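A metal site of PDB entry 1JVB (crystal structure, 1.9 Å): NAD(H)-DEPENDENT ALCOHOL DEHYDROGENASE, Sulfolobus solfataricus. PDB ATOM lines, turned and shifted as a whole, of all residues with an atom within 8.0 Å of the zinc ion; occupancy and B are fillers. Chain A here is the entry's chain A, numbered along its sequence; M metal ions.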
ATOM      1  N   GLY A  36     -10.896 -19.779   8.898  1.00  0.00           N
ATOM      2  CA  GLY A  36     -10.356 -21.115   9.048  1.00  0.00           C
ATOM      3  C   GLY A  36      -8.834 -21.112   9.186  1.00  0.00           C
ATOM      4  O   GLY A  36      -8.125 -20.237   8.651  1.00  0.00           O
ATOM      5  N   VAL A  37      -8.326 -22.106   9.920  1.00  0.00           N
ATOM      6  CA  VAL A  37      -6.873 -22.271  10.090  1.00  0.00           C
ATOM      7  C   VAL A  37      -6.497 -23.689   9.564  1.00  0.00           C
ATOM      8  O   VAL A  37      -7.086 -24.659   9.980  1.00  0.00           O
ATOM      9  CB  VAL A  37      -6.494 -22.179  11.619  1.00  0.00           C
ATOM     10  CG1 VAL A  37      -4.961 -22.350  11.774  1.00  0.00           C
ATOM     11  CG2 VAL A  37      -6.966 -20.825  12.185  1.00  0.00           C
ATOM     12  N   CYS A  38      -5.570 -23.821   8.603  1.00  0.00           N
ATOM     13  CA  CYS A  38      -5.189 -25.172   8.117  1.00  0.00           C
ATOM     14  C   CYS A  38      -3.661 -25.371   8.112  1.00  0.00           C
ATOM     15  O   CYS A  38      -2.929 -24.472   8.476  1.00  0.00           O
ATOM     16  CB  CYS A  38      -5.774 -25.472   6.718  1.00  0.00           C
ATOM     17  SG  CYS A  38      -4.824 -24.764   5.322  1.00  0.00           S
ATOM     18  N   HIS A  39      -3.195 -26.565   7.760  1.00  0.00           N
ATOM     19  CA  HIS A  39      -1.743 -26.854   7.761  1.00  0.00           C
ATOM     20  C   HIS A  39      -0.944 -25.853   6.933  1.00  0.00           C
ATOM     21  O   HIS A  39       0.238 -25.589   7.188  1.00  0.00           O
ATOM     22  CB  HIS A  39      -1.492 -28.285   7.264  1.00  0.00           C
ATOM     23  CG  HIS A  39      -1.601 -29.320   8.338  1.00  0.00           C
ATOM     24  ND1 HIS A  39      -2.727 -30.112   8.507  1.00  0.00           N
ATOM     25  CD2 HIS A  39      -0.755 -29.650   9.352  1.00  0.00           C
ATOM     26  CE1 HIS A  39      -2.577 -30.865   9.586  1.00  0.00           C
ATOM     27  NE2 HIS A  39      -1.391 -30.603  10.114  1.00  0.00           N
ATOM     28  N   SER A  40      -1.583 -25.241   5.929  1.00  0.00           N
ATOM     29  CA  SER A  40      -0.867 -24.235   5.138  1.00  0.00           C
ATOM     30  C   SER A  40      -0.434 -23.100   6.042  1.00  0.00           C
ATOM     31  O   SER A  40       0.565 -22.418   5.765  1.00  0.00           O
ATOM     32  CB  SER A  40      -1.772 -23.672   4.024  1.00  0.00           C
ATOM     33  OG  SER A  40      -2.083 -24.685   3.104  1.00  0.00           O
ATOM     34  N   ASP A  41      -1.148 -22.843   7.144  1.00  0.00           N
ATOM     35  CA  ASP A  41      -0.712 -21.750   7.961  1.00  0.00           C
ATOM     36  C   ASP A  41       0.520 -22.054   8.818  1.00  0.00           C
ATOM     37  O   ASP A  41       1.188 -21.129   9.299  1.00  0.00           O
ATOM     38  CB  ASP A  41      -1.854 -21.215   8.798  1.00  0.00           C
ATOM     39  CG  ASP A  41      -2.914 -20.533   7.926  1.00  0.00           C
ATOM     40  OD1 ASP A  41      -2.496 -19.834   6.986  1.00  0.00           O
ATOM     41  OD2 ASP A  41      -4.117 -20.712   8.170  1.00  0.00           O
ATOM     42  N   PHE A  49       4.854 -20.788   1.129  1.00  0.00           N
ATOM     43  CA  PHE A  49       3.624 -21.411   0.616  1.00  0.00           C
ATOM     44  C   PHE A  49       4.212 -22.490  -0.296  1.00  0.00           C
ATOM     45  O   PHE A  49       4.736 -22.167  -1.357  1.00  0.00           O
ATOM     46  CB  PHE A  49       2.791 -20.447  -0.234  1.00  0.00           C
ATOM     47  CG  PHE A  49       1.489 -21.057  -0.713  1.00  0.00           C
ATOM     48  CD1 PHE A  49       0.399 -21.182   0.151  1.00  0.00           C
ATOM     49  CD2 PHE A  49       1.399 -21.601  -2.003  1.00  0.00           C
ATOM     50  CE1 PHE A  49      -0.781 -21.860  -0.252  1.00  0.00           C
ATOM     51  CE2 PHE A  49       0.212 -22.273  -2.421  1.00  0.00           C
ATOM     52  CZ  PHE A  49      -0.882 -22.399  -1.534  1.00  0.00           C
ATOM     53  N   GLY A  67      -4.865 -15.786   6.897  1.00  0.00           N
ATOM     54  CA  GLY A  67      -6.266 -16.198   6.872  1.00  0.00           C
ATOM     55  C   GLY A  67      -6.837 -16.233   5.454  1.00  0.00           C
ATOM     56  O   GLY A  67      -7.402 -15.246   4.977  1.00  0.00           O
ATOM     57  N   HIS A  68      -6.694 -17.382   4.818  1.00  0.00           N
ATOM     58  CA  HIS A  68      -7.191 -17.592   3.469  1.00  0.00           C
ATOM     59  C   HIS A  68      -8.505 -18.372   3.439  1.00  0.00           C
ATOM     60  O   HIS A  68      -8.966 -18.659   2.356  1.00  0.00           O
ATOM     61  CB  HIS A  68      -6.145 -18.329   2.635  1.00  0.00           C
ATOM     62  CG  HIS A  68      -5.713 -19.658   3.225  1.00  0.00           C
ATOM     63  ND1 HIS A  68      -4.772 -19.789   4.222  1.00  0.00           N
ATOM     64  CD2 HIS A  68      -6.208 -20.906   3.018  1.00  0.00           C
ATOM     65  CE1 HIS A  68      -4.754 -21.082   4.604  1.00  0.00           C
ATOM     66  NE2 HIS A  68      -5.609 -21.812   3.904  1.00  0.00           N
ATOM     67  N   GLU A  69      -9.101 -18.703   4.587  1.00  0.00           N
ATOM     68  CA  GLU A  69     -10.354 -19.458   4.640  1.00  0.00           C
ATOM     69  C   GLU A  69     -11.357 -18.473   5.283  1.00  0.00           C
ATOM     70  O   GLU A  69     -11.446 -18.365   6.526  1.00  0.00           O
ATOM     71  CB  GLU A  69     -10.179 -20.727   5.499  1.00  0.00           C
ATOM     72  CG  GLU A  69      -9.135 -21.655   4.915  1.00  0.00           C
ATOM     73  CD  GLU A  69      -9.009 -22.981   5.635  1.00  0.00           C
ATOM     74  OE1 GLU A  69      -9.804 -23.283   6.583  1.00  0.00           O
ATOM     75  OE2 GLU A  69      -8.144 -23.800   5.226  1.00  0.00           O
ATOM     76  N   PRO A  94     -10.504 -16.970  -2.200  1.00  0.00           N
ATOM     77  CA  PRO A  94      -9.284 -16.210  -2.050  1.00  0.00           C
ATOM     78  C   PRO A  94      -8.220 -16.344  -3.161  1.00  0.00           C
ATOM     79  O   PRO A  94      -7.211 -15.632  -3.149  1.00  0.00           O
ATOM     80  CB  PRO A  94      -8.724 -16.754  -0.726  1.00  0.00           C
ATOM     81  CG  PRO A  94      -9.003 -18.249  -0.874  1.00  0.00           C
ATOM     82  CD  PRO A  94     -10.444 -18.254  -1.444  1.00  0.00           C
ATOM     83  N   TRP A  95      -8.439 -17.281  -4.094  1.00  0.00           N
ATOM     84  CA  TRP A  95      -7.415 -17.595  -5.110  1.00  0.00           C
ATOM     85  C   TRP A  95      -7.699 -16.750  -6.326  1.00  0.00           C
ATOM     86  O   TRP A  95      -8.148 -17.244  -7.366  1.00  0.00           O
ATOM     87  CB  TRP A  95      -7.517 -19.124  -5.408  1.00  0.00           C
ATOM     88  CG  TRP A  95      -7.585 -19.966  -4.114  1.00  0.00           C
ATOM     89  CD1 TRP A  95      -8.665 -20.654  -3.657  1.00  0.00           C
ATOM     90  CD2 TRP A  95      -6.580 -20.098  -3.102  1.00  0.00           C
ATOM     91  NE1 TRP A  95      -8.404 -21.207  -2.424  1.00  0.00           N
ATOM     92  CE2 TRP A  95      -7.134 -20.873  -2.051  1.00  0.00           C
ATOM     93  CE3 TRP A  95      -5.267 -19.630  -2.976  1.00  0.00           C
ATOM     94  CZ2 TRP A  95      -6.411 -21.191  -0.876  1.00  0.00           C
ATOM     95  CZ3 TRP A  95      -4.542 -19.969  -1.769  1.00  0.00           C
ATOM     96  CH2 TRP A  95      -5.135 -20.738  -0.766  1.00  0.00           C
ATOM     97  N   ILE A 120      -2.413 -15.033   1.930  1.00  0.00           N
ATOM     98  CA  ILE A 120      -1.098 -15.550   1.504  1.00  0.00           C
ATOM     99  C   ILE A 120      -0.151 -14.388   1.098  1.00  0.00           C
ATOM    100  O   ILE A 120       0.885 -14.134   1.763  1.00  0.00           O
ATOM    101  CB  ILE A 120      -1.224 -16.563   0.330  1.00  0.00           C
ATOM    102  CG1 ILE A 120      -2.188 -17.717   0.679  1.00  0.00           C
ATOM    103  CG2 ILE A 120       0.166 -17.084  -0.039  1.00  0.00           C
ATOM    104  CD1 ILE A 120      -1.842 -18.541   1.929  1.00  0.00           C
ATOM    105  N   ALA A 150     -16.456 -21.441   5.721  1.00  0.00           N
ATOM    106  CA  ALA A 150     -15.060 -21.021   5.574  1.00  0.00           C
ATOM    107  C   ALA A 150     -13.998 -22.048   5.125  1.00  0.00           C
ATOM    108  O   ALA A 150     -13.204 -21.754   4.236  1.00  0.00           O
ATOM    109  CB  ALA A 150     -14.577 -20.314   6.823  1.00  0.00           C
ATOM    110  N   PRO A 151     -13.975 -23.247   5.729  1.00  0.00           N
ATOM    111  CA  PRO A 151     -12.976 -24.276   5.351  1.00  0.00           C
ATOM    112  C   PRO A 151     -13.123 -24.739   3.883  1.00  0.00           C
ATOM    113  O   PRO A 151     -12.161 -25.163   3.269  1.00  0.00           O
ATOM    114  CB  PRO A 151     -13.262 -25.417   6.351  1.00  0.00           C
ATOM    115  CG  PRO A 151     -13.872 -24.699   7.562  1.00  0.00           C
ATOM    116  CD  PRO A 151     -14.786 -23.666   6.896  1.00  0.00           C
ATOM    117  N   LEU A 152     -14.338 -24.667   3.359  1.00  0.00           N
ATOM    118  CA  LEU A 152     -14.638 -25.083   1.985  1.00  0.00           C
ATOM    119  C   LEU A 152     -13.904 -24.269   0.925  1.00  0.00           C
ATOM    120  O   LEU A 152     -13.695 -24.736  -0.212  1.00  0.00           O
ATOM    121  CB  LEU A 152     -16.142 -24.995   1.767  1.00  0.00           C
ATOM    122  CG  LEU A 152     -17.094 -26.186   1.999  1.00  0.00           C
ATOM    123  CD1 LEU A 152     -16.543 -27.281   2.945  1.00  0.00           C
ATOM    124  CD2 LEU A 152     -18.413 -25.598   2.436  1.00  0.00           C
ATOM    125  N   THR A 153     -13.558 -23.030   1.270  1.00  0.00           N
ATOM    126  CA  THR A 153     -12.850 -22.125   0.350  1.00  0.00           C
ATOM    127  C   THR A 153     -11.430 -22.566   0.103  1.00  0.00           C
ATOM    128  O   THR A 153     -10.712 -21.978  -0.728  1.00  0.00           O
ATOM    129  CB  THR A 153     -12.788 -20.690   0.909  1.00  0.00           C
ATOM    130  OG1 THR A 153     -11.972 -20.685   2.099  1.00  0.00           O
ATOM    131  CG2 THR A 153     -14.165 -20.189   1.229  1.00  0.00           C
ATOM    132  N   CYS A 154     -10.964 -23.563   0.871  1.00  0.00           N
ATOM    133  CA  CYS A 154      -9.607 -24.054   0.703  1.00  0.00           C
ATOM    134  C   CYS A 154      -9.649 -25.580   0.543  1.00  0.00           C
ATOM    135  O   CYS A 154      -9.264 -26.137  -0.504  1.00  0.00           O
ATOM    136  CB  CYS A 154      -8.753 -23.652   1.925  1.00  0.00           C
ATOM    137  SG  CYS A 154      -7.065 -24.336   1.967  1.00  0.00           S
ATOM    138  N   SER A 155     -10.116 -26.280   1.589  1.00  0.00           N
ATOM    139  CA  SER A 155     -10.155 -27.735   1.518  1.00  0.00           C
ATOM    140  C   SER A 155     -11.204 -28.228   0.573  1.00  0.00           C
ATOM    141  O   SER A 155     -11.009 -29.246  -0.094  1.00  0.00           O
ATOM    142  CB  SER A 155     -10.403 -28.342   2.895  1.00  0.00           C
ATOM    143  OG  SER A 155      -9.352 -27.928   3.751  1.00  0.00           O
ATOM    144  N   GLY A 156     -12.333 -27.543   0.547  1.00  0.00           N
ATOM    145  CA  GLY A 156     -13.403 -27.983  -0.318  1.00  0.00           C
ATOM    146  C   GLY A 156     -13.017 -27.763  -1.773  1.00  0.00           C
ATOM    147  O   GLY A 156     -13.154 -28.634  -2.594  1.00  0.00           O
ATOM    148  N   THR A 158     -10.040 -27.374  -3.091  1.00  0.00           N
ATOM    149  CA  THR A 158      -8.880 -28.180  -3.459  1.00  0.00           C
ATOM    150  C   THR A 158      -9.265 -29.618  -3.814  1.00  0.00           C
ATOM    151  O   THR A 158      -8.834 -30.144  -4.871  1.00  0.00           O
ATOM    152  CB  THR A 158      -7.825 -28.193  -2.311  1.00  0.00           C
ATOM    153  OG1 THR A 158      -7.249 -26.882  -2.179  1.00  0.00           O
ATOM    154  CG2 THR A 158      -6.653 -29.171  -2.649  1.00  0.00           C
ATOM    155  N   LEU A 183      -9.238 -33.649   4.945  1.00  0.00           N
ATOM    156  CA  LEU A 183      -9.148 -33.502   3.500  1.00  0.00           C
ATOM    157  C   LEU A 183      -9.627 -34.763   2.805  1.00  0.00           C
ATOM    158  O   LEU A 183     -10.364 -34.709   1.821  1.00  0.00           O
ATOM    159  CB  LEU A 183      -7.708 -33.217   3.109  1.00  0.00           C
ATOM    160  CG  LEU A 183      -7.375 -32.222   2.012  1.00  0.00           C
ATOM    161  CD1 LEU A 183      -7.955 -30.876   2.359  1.00  0.00           C
ATOM    162  CD2 LEU A 183      -5.866 -32.076   1.886  1.00  0.00           C
ATOM    163  N   VAL A 296      -5.429 -25.796  -5.324  1.00  0.00           N
ATOM    164  CA  VAL A 296      -6.647 -25.081  -4.950  1.00  0.00           C
ATOM    165  C   VAL A 296      -7.716 -25.195  -6.042  1.00  0.00           C
ATOM    166  O   VAL A 296      -8.116 -26.314  -6.414  1.00  0.00           O
ATOM    167  CB  VAL A 296      -6.356 -23.546  -4.557  1.00  0.00           C
ATOM    168  CG1 VAL A 296      -5.400 -23.498  -3.301  1.00  0.00           C
ATOM    169  CG2 VAL A 296      -5.663 -22.814  -5.673  1.00  0.00           C
ATOM    170  N   ARG A 342     -11.192 -29.210  12.118  1.00  0.00           N
ATOM    171  CA  ARG A 342     -10.702 -27.955  11.534  1.00  0.00           C
ATOM    172  C   ARG A 342     -10.966 -26.793  12.481  1.00  0.00           C
ATOM    173  O   ARG A 342     -12.122 -26.525  12.842  1.00  0.00           O
ATOM    174  CB  ARG A 342     -11.418 -27.717  10.198  1.00  0.00           C
ATOM    175  CG  ARG A 342     -11.217 -26.322   9.608  1.00  0.00           C
ATOM    176  CD  ARG A 342      -9.782 -26.011   9.285  1.00  0.00           C
ATOM    177  NE  ARG A 342      -9.144 -27.079   8.532  1.00  0.00           N
ATOM    178  CZ  ARG A 342      -9.092 -27.182   7.207  1.00  0.00           C
ATOM    179  NH1 ARG A 342      -9.659 -26.257   6.423  1.00  0.00           N
ATOM    180  NH2 ARG A 342      -8.539 -28.257   6.657  1.00  0.00           N
HETATM  181 ZN    ZN M   1      -6.486 -23.653   4.094  1.00  0.00          ZN
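The zinc ion is bound by OE2 of Glu 69, NE2 of His 68, SG of Cys 154 and SG of Cys 38.
The zinc ion has four donor atoms within binding distance.
Of the 24 residues printed, 4 come within 4 Å of the zinc ion.
The nearest printed residue that does not touch the zinc ion is Ser 40 (4.6 Å).
NH1 of Arg 342 is in salt-bridge range of OE1 of Glu 69 (3.0 Å).
N of Gly 36 is in hydrogen-bond range of O of Glu 69, at 2.8 Å.
The side-chain hydroxyl (OG1) of Thr 158 is in hydrogen-bond range of the backbone carbonyl oxygen (O) of Cys 154, at 2.7 Å.
The side-chain sulfur (SG) of Cys 38 lies close to the backbone NH (N) of Ser 40, at 3.3 Å.
The backbone NH (N) of Cys 38 sits at hydrogen-bond distance from the side-chain carboxylate (OD2) of Asp 41, 3.5 Å away.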
